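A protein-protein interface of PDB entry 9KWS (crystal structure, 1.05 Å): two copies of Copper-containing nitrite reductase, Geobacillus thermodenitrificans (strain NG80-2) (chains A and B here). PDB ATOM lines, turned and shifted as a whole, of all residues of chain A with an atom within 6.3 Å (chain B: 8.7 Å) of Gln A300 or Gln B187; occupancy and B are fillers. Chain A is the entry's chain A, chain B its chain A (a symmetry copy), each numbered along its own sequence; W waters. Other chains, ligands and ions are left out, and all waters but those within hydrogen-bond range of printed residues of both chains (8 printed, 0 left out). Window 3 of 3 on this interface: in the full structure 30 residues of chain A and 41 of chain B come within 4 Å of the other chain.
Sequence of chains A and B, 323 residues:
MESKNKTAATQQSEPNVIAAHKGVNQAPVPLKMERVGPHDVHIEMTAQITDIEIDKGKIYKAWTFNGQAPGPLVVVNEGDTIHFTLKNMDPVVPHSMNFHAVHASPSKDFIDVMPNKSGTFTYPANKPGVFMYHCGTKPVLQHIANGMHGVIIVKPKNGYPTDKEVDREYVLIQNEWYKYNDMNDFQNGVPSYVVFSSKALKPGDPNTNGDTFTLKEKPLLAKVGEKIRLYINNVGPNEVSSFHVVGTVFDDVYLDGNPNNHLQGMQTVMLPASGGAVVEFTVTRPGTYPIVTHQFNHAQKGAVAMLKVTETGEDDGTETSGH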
ATOM      1  N   VAL A 190       6.482  -2.581  31.159  1.00  0.00           N
ATOM      2  CA  VAL A 190       7.457  -2.587  30.072  1.00  0.00           C
ATOM      3  C   VAL A 190       8.519  -3.646  30.338  1.00  0.00           C
ATOM      4  O   VAL A 190       8.820  -3.959  31.505  1.00  0.00           O
ATOM      5  CB  VAL A 190       8.107  -1.206  29.870  1.00  0.00           C
ATOM      6  CG1 VAL A 190       7.073  -0.171  29.454  1.00  0.00           C
ATOM      7  CG2 VAL A 190       8.895  -0.768  31.112  1.00  0.00           C
ATOM      8  N   PRO A 191       9.147  -4.183  29.301  1.00  0.00           N
ATOM      9  CA  PRO A 191      10.235  -5.142  29.534  1.00  0.00           C
ATOM     10  C   PRO A 191      11.405  -4.468  30.226  1.00  0.00           C
ATOM     11  O   PRO A 191      11.740  -3.318  29.947  1.00  0.00           O
ATOM     12  CB  PRO A 191      10.597  -5.605  28.120  1.00  0.00           C
ATOM     13  CG  PRO A 191      10.125  -4.525  27.221  1.00  0.00           C
ATOM     14  CD  PRO A 191       8.900  -3.970  27.867  1.00  0.00           C
ATOM     15  N   GLN A 295      13.053  -0.334  17.327  1.00  0.00           N
ATOM     16  CA  GLN A 295      12.329   0.223  18.468  1.00  0.00           C
ATOM     17  C   GLN A 295      13.399   0.501  19.517  1.00  0.00           C
ATOM     18  O   GLN A 295      13.852  -0.411  20.214  1.00  0.00           O
ATOM     19  CB  GLN A 295      11.259  -0.758  18.905  1.00  0.00           C
ATOM     20  CG  GLN A 295      10.148  -0.862  17.837  1.00  0.00           C
ATOM     21  CD  GLN A 295       9.375  -2.157  17.891  1.00  0.00           C
ATOM     22  OE1 GLN A 295       9.303  -2.887  16.907  1.00  0.00           O
ATOM     23  NE2 GLN A 295       8.769  -2.446  19.041  1.00  0.00           N
ATOM     24  N   PHE A 296      13.893   1.740  19.538  1.00  0.00           N
ATOM     25  CA  PHE A 296      15.181   1.988  20.183  1.00  0.00           C
ATOM     26  C   PHE A 296      15.119   1.941  21.700  1.00  0.00           C
ATOM     27  O   PHE A 296      16.165   1.772  22.338  1.00  0.00           O
ATOM     28  CB  PHE A 296      15.881   3.246  19.628  1.00  0.00           C
ATOM     29  CG  PHE A 296      17.033   2.874  18.738  1.00  0.00           C
ATOM     30  CD1 PHE A 296      18.263   2.560  19.292  1.00  0.00           C
ATOM     31  CD2 PHE A 296      16.858   2.708  17.371  1.00  0.00           C
ATOM     32  CE1 PHE A 296      19.293   2.101  18.486  1.00  0.00           C
ATOM     33  CE2 PHE A 296      17.889   2.251  16.568  1.00  0.00           C
ATOM     34  CZ  PHE A 296      19.100   1.943  17.124  1.00  0.00           C
ATOM     35  N   ASN A 297      13.933   2.030  22.297  1.00  0.00           N
ATOM     36  CA  ASN A 297      13.819   1.738  23.717  1.00  0.00           C
ATOM     37  C   ASN A 297      14.245   0.309  24.019  1.00  0.00           C
ATOM     38  O   ASN A 297      14.933   0.054  25.017  1.00  0.00           O
ATOM     39  CB  ASN A 297      12.423   2.077  24.264  1.00  0.00           C
ATOM     40  CG  ASN A 297      11.242   1.462  23.511  1.00  0.00           C
ATOM     41  OD1 ASN A 297      11.348   0.836  22.482  1.00  0.00           O
ATOM     42  ND2 ASN A 297      10.059   1.734  24.041  1.00  0.00           N
ATOM     43  N   HIS A 298      13.865  -0.631  23.158  1.00  0.00           N
ATOM     44  CA  HIS A 298      14.251  -2.029  23.315  1.00  0.00           C
ATOM     45  C   HIS A 298      15.731  -2.228  23.022  1.00  0.00           C
ATOM     46  O   HIS A 298      16.413  -2.981  23.727  1.00  0.00           O
ATOM     47  CB  HIS A 298      13.390  -2.901  22.416  1.00  0.00           C
ATOM     48  CG  HIS A 298      11.936  -2.819  22.724  1.00  0.00           C
ATOM     49  ND1 HIS A 298      10.984  -3.305  21.859  1.00  0.00           N
ATOM     50  CD2 HIS A 298      11.277  -2.300  23.791  1.00  0.00           C
ATOM     51  CE1 HIS A 298       9.794  -3.082  22.388  1.00  0.00           C
ATOM     52  NE2 HIS A 298       9.940  -2.486  23.560  1.00  0.00           N
ATOM     53  N   ALA A 299      16.247  -1.573  21.979  1.00  0.00           N
ATOM     54  CA  ALA A 299      17.677  -1.625  21.704  1.00  0.00           C
ATOM     55  C   ALA A 299      18.481  -1.129  22.900  1.00  0.00           C
ATOM     56  O   ALA A 299      19.480  -1.752  23.291  1.00  0.00           O
ATOM     57  CB  ALA A 299      17.992  -0.813  20.451  1.00  0.00           C
ATOM     58  N   GLN A 300      18.054  -0.019  23.506  1.00  0.00           N
ATOM     59  CA  GLN A 300      18.761   0.519  24.654  1.00  0.00           C
ATOM     60  C   GLN A 300      18.744  -0.447  25.826  1.00  0.00           C
ATOM     61  O   GLN A 300      19.696  -0.474  26.615  1.00  0.00           O
ATOM     62  CB  GLN A 300      18.141   1.859  25.044  1.00  0.00           C
ATOM     63  CG  GLN A 300      18.767   2.506  26.272  1.00  0.00           C
ATOM     64  CD  GLN A 300      20.234   2.843  26.104  1.00  0.00           C
ATOM     65  OE1 GLN A 300      20.725   3.084  25.004  1.00  0.00           O
ATOM     66  NE2 GLN A 300      20.947   2.875  27.224  1.00  0.00           N
ATOM     67  N   LYS A 301      17.672  -1.224  25.962  1.00  0.00           N
ATOM     68  CA  LYS A 301      17.516  -2.200  27.029  1.00  0.00           C
ATOM     69  C   LYS A 301      18.111  -3.560  26.684  1.00  0.00           C
ATOM     70  O   LYS A 301      17.839  -4.537  27.388  1.00  0.00           O
ATOM     71  CB  LYS A 301      16.049  -2.278  27.466  1.00  0.00           C
ATOM     72  CG  LYS A 301      15.632  -0.978  28.177  1.00  0.00           C
ATOM     73  CD  LYS A 301      14.297  -0.981  28.869  1.00  0.00           C
ATOM     74  CE  LYS A 301      13.138  -0.917  27.916  1.00  0.00           C
ATOM     75  NZ  LYS A 301      11.850  -0.793  28.702  1.00  0.00           N
ATOM     76  N   GLY A 302      18.959  -3.625  25.651  1.00  0.00           N
ATOM     77  CA  GLY A 302      19.792  -4.778  25.414  1.00  0.00           C
ATOM     78  C   GLY A 302      19.819  -5.315  24.007  1.00  0.00           C
ATOM     79  O   GLY A 302      20.713  -6.106  23.690  1.00  0.00           O
ATOM     80  N   ALA A 303      18.864  -4.915  23.163  1.00  0.00           N
ATOM     81  CA  ALA A 303      18.622  -5.630  21.908  1.00  0.00           C
ATOM     82  C   ALA A 303      19.477  -5.058  20.776  1.00  0.00           C
ATOM     83  O   ALA A 303      18.990  -4.497  19.790  1.00  0.00           O
ATOM     84  CB  ALA A 303      17.144  -5.634  21.567  1.00  0.00           C
ATOM     85  N   VAL A 304      20.790  -5.236  20.951  1.00  0.00           N
ATOM     86  CA  VAL A 304      21.810  -4.914  19.961  1.00  0.00           C
ATOM     87  C   VAL A 304      22.807  -6.068  19.967  1.00  0.00           C
ATOM     88  O   VAL A 304      23.382  -6.402  21.015  1.00  0.00           O
ATOM     89  CB  VAL A 304      22.541  -3.590  20.245  1.00  0.00           C
ATOM     90  CG1 VAL A 304      23.598  -3.341  19.172  1.00  0.00           C
ATOM     91  CG2 VAL A 304      21.557  -2.434  20.311  1.00  0.00           C
ATOM     92  N   THR B 137      25.195   8.127  17.220  1.00  0.00           N
ATOM     93  CA  THR B 137      26.081   8.270  18.367  1.00  0.00           C
ATOM     94  C   THR B 137      25.449   7.628  19.599  1.00  0.00           C
ATOM     95  O   THR B 137      24.253   7.783  19.861  1.00  0.00           O
ATOM     96  CB  THR B 137      26.363   9.757  18.584  1.00  0.00           C
ATOM     97  OG1 THR B 137      27.004  10.281  17.405  1.00  0.00           O
ATOM     98  CG2 THR B 137      27.244  10.019  19.791  1.00  0.00           C
ATOM     99  N   LYS B 138      26.268   6.902  20.357  1.00  0.00           N
ATOM    100  CA  LYS B 138      25.767   6.213  21.539  1.00  0.00           C
ATOM    101  C   LYS B 138      25.478   7.226  22.645  1.00  0.00           C
ATOM    102  O   LYS B 138      26.270   8.149  22.855  1.00  0.00           O
ATOM    103  CB  LYS B 138      26.813   5.207  22.023  1.00  0.00           C
ATOM    104  CG  LYS B 138      26.655   4.772  23.471  1.00  0.00           C
ATOM    105  CD  LYS B 138      27.294   3.420  23.748  1.00  0.00           C
ATOM    106  CE  LYS B 138      26.719   2.829  25.028  1.00  0.00           C
ATOM    107  NZ  LYS B 138      25.453   3.533  25.422  1.00  0.00           N
ATOM    108  N   PRO B 139      24.350   7.094  23.368  1.00  0.00           N
ATOM    109  CA  PRO B 139      23.258   6.133  23.163  1.00  0.00           C
ATOM    110  C   PRO B 139      22.361   6.587  22.020  1.00  0.00           C
ATOM    111  O   PRO B 139      21.842   7.704  22.026  1.00  0.00           O
ATOM    112  CB  PRO B 139      22.475   6.180  24.484  1.00  0.00           C
ATOM    113  CG  PRO B 139      23.211   7.097  25.381  1.00  0.00           C
ATOM    114  CD  PRO B 139      24.118   7.931  24.555  1.00  0.00           C
ATOM    115  N   VAL B 140      22.176   5.718  21.033  1.00  0.00           N
ATOM    116  CA  VAL B 140      21.448   6.112  19.832  1.00  0.00           C
ATOM    117  C   VAL B 140      20.024   6.525  20.171  1.00  0.00           C
ATOM    118  O   VAL B 140      19.499   7.482  19.599  1.00  0.00           O
ATOM    119  CB  VAL B 140      21.517   4.992  18.780  1.00  0.00           C
ATOM    120  CG1 VAL B 140      20.646   5.309  17.586  1.00  0.00           C
ATOM    121  CG2 VAL B 140      22.960   4.787  18.340  1.00  0.00           C
ATOM    122  N   LEU B 141      19.384   5.836  21.124  1.00  0.00           N
ATOM    123  CA  LEU B 141      18.041   6.235  21.534  1.00  0.00           C
ATOM    124  C   LEU B 141      17.986   7.708  21.924  1.00  0.00           C
ATOM    125  O   LEU B 141      17.021   8.410  21.603  1.00  0.00           O
ATOM    126  CB  LEU B 141      17.582   5.386  22.716  1.00  0.00           C
ATOM    127  CG  LEU B 141      16.280   5.816  23.408  1.00  0.00           C
ATOM    128  CD1 LEU B 141      15.082   5.761  22.478  1.00  0.00           C
ATOM    129  CD2 LEU B 141      16.063   4.950  24.640  1.00  0.00           C
ATOM    130  N   GLN B 142      18.986   8.174  22.665  1.00  0.00           N
ATOM    131  CA  GLN B 142      18.999   9.568  23.107  1.00  0.00           C
ATOM    132  C   GLN B 142      19.096  10.532  21.931  1.00  0.00           C
ATOM    133  O   GLN B 142      18.391  11.552  21.879  1.00  0.00           O
ATOM    134  CB  GLN B 142      20.172   9.775  24.064  1.00  0.00           C
ATOM    135  CG  GLN B 142      20.225  11.158  24.672  1.00  0.00           C
ATOM    136  CD  GLN B 142      21.324  11.301  25.693  1.00  0.00           C
ATOM    137  OE1 GLN B 142      22.265  10.513  25.725  1.00  0.00           O
ATOM    138  NE2 GLN B 142      21.206  12.310  26.538  1.00  0.00           N
ATOM    139  N   HIS B 143      19.970  10.229  20.977  1.00  0.00           N
ATOM    140  CA  HIS B 143      20.146  11.126  19.843  1.00  0.00           C
ATOM    141  C   HIS B 143      18.912  11.132  18.944  1.00  0.00           C
ATOM    142  O   HIS B 143      18.451  12.214  18.517  1.00  0.00           O
ATOM    143  CB  HIS B 143      21.422  10.757  19.112  1.00  0.00           C
ATOM    144  CG  HIS B 143      22.655  11.106  19.888  1.00  0.00           C
ATOM    145  ND1 HIS B 143      23.445  12.183  19.564  1.00  0.00           N
ATOM    146  CD2 HIS B 143      23.210  10.550  20.994  1.00  0.00           C
ATOM    147  CE1 HIS B 143      24.447  12.262  20.420  1.00  0.00           C
ATOM    148  NE2 HIS B 143      24.329  11.285  21.299  1.00  0.00           N
ATOM    149  N   ALA B 145      15.762  10.293  19.882  1.00  0.00           N
ATOM    150  CA  ALA B 145      14.614  10.864  20.586  1.00  0.00           C
ATOM    151  C   ALA B 145      14.704  12.383  20.696  1.00  0.00           C
ATOM    152  O   ALA B 145      13.681  13.069  20.661  1.00  0.00           O
ATOM    153  CB  ALA B 145      14.480  10.242  21.970  1.00  0.00           C
ATOM    154  N   TYR B 178       9.258  12.922  23.629  1.00  0.00           N
ATOM    155  CA  TYR B 178       9.228  12.483  25.020  1.00  0.00           C
ATOM    156  C   TYR B 178       9.555  13.664  25.939  1.00  0.00           C
ATOM    157  O   TYR B 178       9.769  14.794  25.487  1.00  0.00           O
ATOM    158  CB  TYR B 178      10.227  11.317  25.212  1.00  0.00           C
ATOM    159  CG  TYR B 178       9.789  10.077  24.473  1.00  0.00           C
ATOM    160  CD1 TYR B 178      10.077   9.905  23.131  1.00  0.00           C
ATOM    161  CD2 TYR B 178       9.041   9.096  25.111  1.00  0.00           C
ATOM    162  CE1 TYR B 178       9.601   8.817  22.426  1.00  0.00           C
ATOM    163  CE2 TYR B 178       8.559   8.003  24.419  1.00  0.00           C
ATOM    164  CZ  TYR B 178       8.816   7.879  23.081  1.00  0.00           C
ATOM    165  OH  TYR B 178       8.282   6.797  22.410  1.00  0.00           O
ATOM    166  N   LYS B 179       9.598  13.402  27.241  1.00  0.00           N
ATOM    167  CA  LYS B 179      10.102  14.390  28.181  1.00  0.00           C
ATOM    168  C   LYS B 179      11.538  14.748  27.831  1.00  0.00           C
ATOM    169  O   LYS B 179      12.330  13.895  27.439  1.00  0.00           O
ATOM    170  CB  LYS B 179       9.990  13.889  29.612  1.00  0.00           C
ATOM    171  CG  LYS B 179       8.586  13.514  30.039  1.00  0.00           C
ATOM    172  CD  LYS B 179       8.570  12.832  31.410  1.00  0.00           C
ATOM    173  CE  LYS B 179       7.174  12.402  31.788  1.00  0.00           C
ATOM    174  NZ  LYS B 179       7.160  11.738  33.110  1.00  0.00           N
ATOM    175  N   ASP B 182      15.272  12.961  28.593  1.00  0.00           N
ATOM    176  CA  ASP B 182      15.036  12.134  29.778  1.00  0.00           C
ATOM    177  C   ASP B 182      15.168  10.670  29.372  1.00  0.00           C
ATOM    178  O   ASP B 182      14.226  10.077  28.851  1.00  0.00           O
ATOM    179  CB  ASP B 182      13.655  12.458  30.340  1.00  0.00           C
ATOM    180  CG  ASP B 182      13.271  11.630  31.547  1.00  0.00           C
ATOM    181  OD1 ASP B 182      13.907  10.593  31.830  1.00  0.00           O
ATOM    182  OD2 ASP B 182      12.258  11.991  32.185  1.00  0.00           O
ATOM    183  N   MET B 183      16.338  10.076  29.619  1.00  0.00           N
ATOM    184  CA  MET B 183      16.586   8.716  29.153  1.00  0.00           C
ATOM    185  C   MET B 183      15.688   7.689  29.831  1.00  0.00           C
ATOM    186  O   MET B 183      15.375   6.660  29.227  1.00  0.00           O
ATOM    187  CB  MET B 183      18.057   8.347  29.340  1.00  0.00           C
ATOM    188  CG  MET B 183      18.944   8.751  28.172  1.00  0.00           C
ATOM    189  SD  MET B 183      18.649   7.764  26.697  1.00  0.00           S
ATOM    190  CE  MET B 183      19.637   6.332  27.053  1.00  0.00           C
ATOM    191  N   ASN B 184      15.263   7.928  31.069  1.00  0.00           N
ATOM    192  CA  ASN B 184      14.315   7.010  31.681  1.00  0.00           C
ATOM    193  C   ASN B 184      12.999   7.021  30.907  1.00  0.00           C
ATOM    194  O   ASN B 184      12.424   5.970  30.600  1.00  0.00           O
ATOM    195  CB  ASN B 184      14.089   7.360  33.138  1.00  0.00           C
ATOM    196  CG  ASN B 184      13.121   6.421  33.769  1.00  0.00           C
ATOM    197  OD1 ASN B 184      13.353   5.214  33.794  1.00  0.00           O
ATOM    198  ND2 ASN B 184      11.984   6.947  34.193  1.00  0.00           N
ATOM    199  N   ASP B 185      12.506   8.214  30.585  1.00  0.00           N
ATOM    200  CA  ASP B 185      11.277   8.322  29.809  1.00  0.00           C
ATOM    201  C   ASP B 185      11.457   7.746  28.413  1.00  0.00           C
ATOM    202  O   ASP B 185      10.570   7.058  27.896  1.00  0.00           O
ATOM    203  CB  ASP B 185      10.832   9.785  29.748  1.00  0.00           C
ATOM    204  CG  ASP B 185       9.396   9.945  29.313  1.00  0.00           C
ATOM    205  OD1 ASP B 185       8.520   9.314  29.951  1.00  0.00           O
ATOM    206  OD2 ASP B 185       9.151  10.707  28.350  1.00  0.00           O
ATOM    207  N   PHE B 186      12.600   8.022  27.782  1.00  0.00           N
ATOM    208  CA  PHE B 186      12.832   7.515  26.440  1.00  0.00           C
ATOM    209  C   PHE B 186      12.727   5.992  26.400  1.00  0.00           C
ATOM    210  O   PHE B 186      12.237   5.423  25.418  1.00  0.00           O
ATOM    211  CB  PHE B 186      14.224   7.896  25.931  1.00  0.00           C
ATOM    212  CG  PHE B 186      14.478   9.376  25.696  1.00  0.00           C
ATOM    213  CD1 PHE B 186      13.483  10.340  25.722  1.00  0.00           C
ATOM    214  CD2 PHE B 186      15.776   9.782  25.407  1.00  0.00           C
ATOM    215  CE1 PHE B 186      13.781  11.667  25.465  1.00  0.00           C
ATOM    216  CE2 PHE B 186      16.071  11.113  25.140  1.00  0.00           C
ATOM    217  CZ  PHE B 186      15.068  12.060  25.169  1.00  0.00           C
ATOM    218  N   GLN B 187      13.243   5.322  27.446  1.00  0.00           N
ATOM    219  CA  GLN B 187      13.300   3.863  27.500  1.00  0.00           C
ATOM    220  C   GLN B 187      11.994   3.237  27.963  1.00  0.00           C
ATOM    221  O   GLN B 187      11.635   2.145  27.503  1.00  0.00           O
ATOM    222  CB  GLN B 187      14.380   3.412  28.487  1.00  0.00           C
ATOM    223  CG  GLN B 187      15.781   3.584  28.010  1.00  0.00           C
ATOM    224  CD  GLN B 187      16.764   3.254  29.101  1.00  0.00           C
ATOM    225  OE1 GLN B 187      17.062   2.088  29.345  1.00  0.00           O
ATOM    226  NE2 GLN B 187      17.239   4.273  29.795  1.00  0.00           N
ATOM    227  N   ASN B 188      11.322   3.881  28.919  1.00  0.00           N
ATOM    228  CA  ASN B 188      10.278   3.253  29.719  1.00  0.00           C
ATOM    229  C   ASN B 188       8.928   3.943  29.673  1.00  0.00           C
ATOM    230  O   ASN B 188       7.958   3.375  30.190  1.00  0.00           O
ATOM    231  CB  ASN B 188      10.726   3.159  31.186  1.00  0.00           C
ATOM    232  CG  ASN B 188      11.936   2.273  31.348  1.00  0.00           C
ATOM    233  OD1 ASN B 188      11.966   1.159  30.833  1.00  0.00           O
ATOM    234  ND2 ASN B 188      12.948   2.765  32.051  1.00  0.00           N
ATOM    235  N   GLY B 189       8.835   5.138  29.102  1.00  0.00           N
ATOM    236  CA  GLY B 189       7.611   5.912  29.144  1.00  0.00           C
ATOM    237  C   GLY B 189       6.865   5.947  27.832  1.00  0.00           C
ATOM    238  O   GLY B 189       7.437   5.769  26.755  1.00  0.00           O
ATOM    239  N   VAL B 190       5.578   6.246  27.902  1.00  0.00           N
ATOM    240  CA  VAL B 190       4.801   6.485  26.689  1.00  0.00           C
ATOM    241  C   VAL B 190       5.214   7.813  26.066  1.00  0.00           C
ATOM    242  O   VAL B 190       5.639   8.741  26.780  1.00  0.00           O
ATOM    243  CB  VAL B 190       3.285   6.461  26.959  1.00  0.00           C
ATOM    244  CG1 VAL B 190       2.836   5.089  27.438  1.00  0.00           C
ATOM    245  CG2 VAL B 190       2.868   7.575  27.929  1.00  0.00           C
ATOM    246  N   PRO B 237      11.226   7.319  17.780  1.00  0.00           N
ATOM    247  CA  PRO B 237      12.181   6.217  17.927  1.00  0.00           C
ATOM    248  C   PRO B 237      11.622   4.854  18.282  1.00  0.00           C
ATOM    249  O   PRO B 237      12.293   3.858  17.995  1.00  0.00           O
ATOM    250  CB  PRO B 237      13.096   6.683  19.082  1.00  0.00           C
ATOM    251  CG  PRO B 237      12.266   7.689  19.823  1.00  0.00           C
ATOM    252  CD  PRO B 237      11.494   8.400  18.747  1.00  0.00           C
ATOM    253  N   ASN B 238      10.454   4.798  18.922  1.00  0.00           N
ATOM    254  CA  ASN B 238      10.050   3.590  19.613  1.00  0.00           C
ATOM    255  C   ASN B 238       8.797   2.921  19.100  1.00  0.00           C
ATOM    256  O   ASN B 238       8.637   1.719  19.326  1.00  0.00           O
ATOM    257  CB  ASN B 238       9.806   3.911  21.092  1.00  0.00           C
ATOM    258  CG  ASN B 238      11.040   4.406  21.780  1.00  0.00           C
ATOM    259  OD1 ASN B 238      12.161   4.038  21.421  1.00  0.00           O
ATOM    260  ND2 ASN B 238      10.857   5.224  22.797  1.00  0.00           N
HETATM  261  O   HOH W   1       8.633   2.102  26.984  1.00  0.00           O
HETATM  262  O   HOH W   2      19.657   1.784  29.749  1.00  0.00           O
HETATM  263  O   HOH W   3      23.276   2.378  24.166  1.00  0.00           O
HETATM  264  O   HOH W   4      20.189   3.300  22.272  1.00  0.00           O
HETATM  265  O   HOH W   5       9.573   4.424  25.756  1.00  0.00           O
HETATM  266  O   HOH W   6      23.589   4.047  27.763  1.00  0.00           O
HETATM  267  O   HOH W   7       9.919  -0.365  26.818  1.00  0.00           O
HETATM  268  O   HOH W   8       8.979  -0.145  21.297  1.00  0.00           O
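The backbone NH of Asn A297 lies within hydrogen-bond range of the side-chain amide oxygen of Asn B238, 2.8 Å away. OD1 of Asn B238 is in hydrogen-bond range of N of Phe A296. The side-chain amino group (NZ) of Lys A301 lies within hydrogen-bond range of the side-chain amide oxygen (OD1) of Asn B188, at 2.9 Å. The side-chain amino group (NZ) of Lys A301 lies within hydrogen-bond range of the backbone carbonyl oxygen (O) of Gln B187 (3.2 Å). N of Phe A296 is in hydrogen-bond range of O of Pro B237, at 3.1 Å.
The side-chain amide nitrogen (NE2) of Gln B187 lies within hydrogen-bond range of the backbone carbonyl oxygen (O) of Met B183. The side-chain amide oxygen (OD1) of Asn B184 sits at hydrogen-bond distance from the side-chain amide nitrogen (ND2) of Asn B188 (3.0 Å). The side-chain amino group of Lys A301 is in hydrogen-bond range of the backbone carbonyl oxygen of Pro A191. O of Phe B186 is in hydrogen-bond range of ND2 of Asn B238, 3.0 Å away. OH of Tyr B178 sits at hydrogen-bond distance from ND2 of Asn B238, at 3.0 Å.
Among the printed residues, pairs that only touch across the chains: Val A190 with Asn B188, Gln A295 with Pro B237, Gln A295 with Asn B238, Phe A296 with Val B140, Phe A296 with Leu B141, Asn A297 with Leu B141, Asn A297 with Phe B186, Asn A297 with Gln B187, Gln A300 with Pro B139, Gln A300 with Leu B141, Gln A300 with Met B183 and Gln A300 with Gln B187.
Of the printed residues of chain B, Asn A297 touches Leu B141 (3.9 Å), Phe B186 (3.5 Å), Gln B187 (3.3 Å) and Asn B238 (2.8 Å). No residue of chain B comes within 4 Å of Ala A299. Of the printed residues of chain B, Gln A300 touches Pro B139 (3.6 Å), Leu B141 (3.7 Å), Met B183 (3.7 Å) and Gln B187 (3.5 Å). Printed residues of chain A within 4 Å of Leu B141: Phe A296, Asn A297 and Gln A300. Printed residues of chain A within 4 Å of Met B183: Gln A300. Printed residues of chain A within 4 Å of Gln B187: Asn A297, Gln A300 and Lys A301. Printed residues of chain A within 4 Å of Asn B188: Val A190 (3.6 Å) and Lys A301 (2.9 Å). The nearest printed residue of chain A that does not touch Gln B187 is Val A190 (5.4 Å). The nearest printed residue of chain A that does not touch Pro B237 is Asn A297 (5.0 Å).
Printed residues of chain A that touch a printed residue of chain B: Val A190, Gln A295, Phe A296, Asn A297, Gln A300 and Lys A301. Among the printed residues, 17 pairs touch across the chains.
Position printed for both chains: 190.
Water W2 bridges the side-chain amide oxygen (OE1) of Gln B187 and the side-chain amide nitrogen (NE2) of Gln A300. Water W5 lies within hydrogen-bond range of the backbone carbonyl oxygen (O) of Gly B189 (2.7 Å), the backbone carbonyl oxygen (O) of Phe B186 (2.9 Å), the side-chain amide nitrogen (ND2) of Asn A297 (3.2 Å) and the side-chain amide nitrogen (ND2) of Asn B238 (3.3 Å). Water W7 lies within hydrogen-bond range of NZ of Lys A301 (2.7 Å), O of Gln B187 (3.1 Å) and ND2 of Asn A297 (3.5 Å). Water W4 lies within hydrogen-bond range of OE1 of Gln A300 (2.8 Å), N of Leu B141 (2.9 Å) and N of Val B140 (3.4 Å). Water W6 lies within hydrogen-bond range of NE2 of Gln A300 (2.9 Å) and NZ of Lys B138 (3.0 Å). Water W1 lies within hydrogen-bond range of O of Gln B187 and ND2 of Asn A297.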
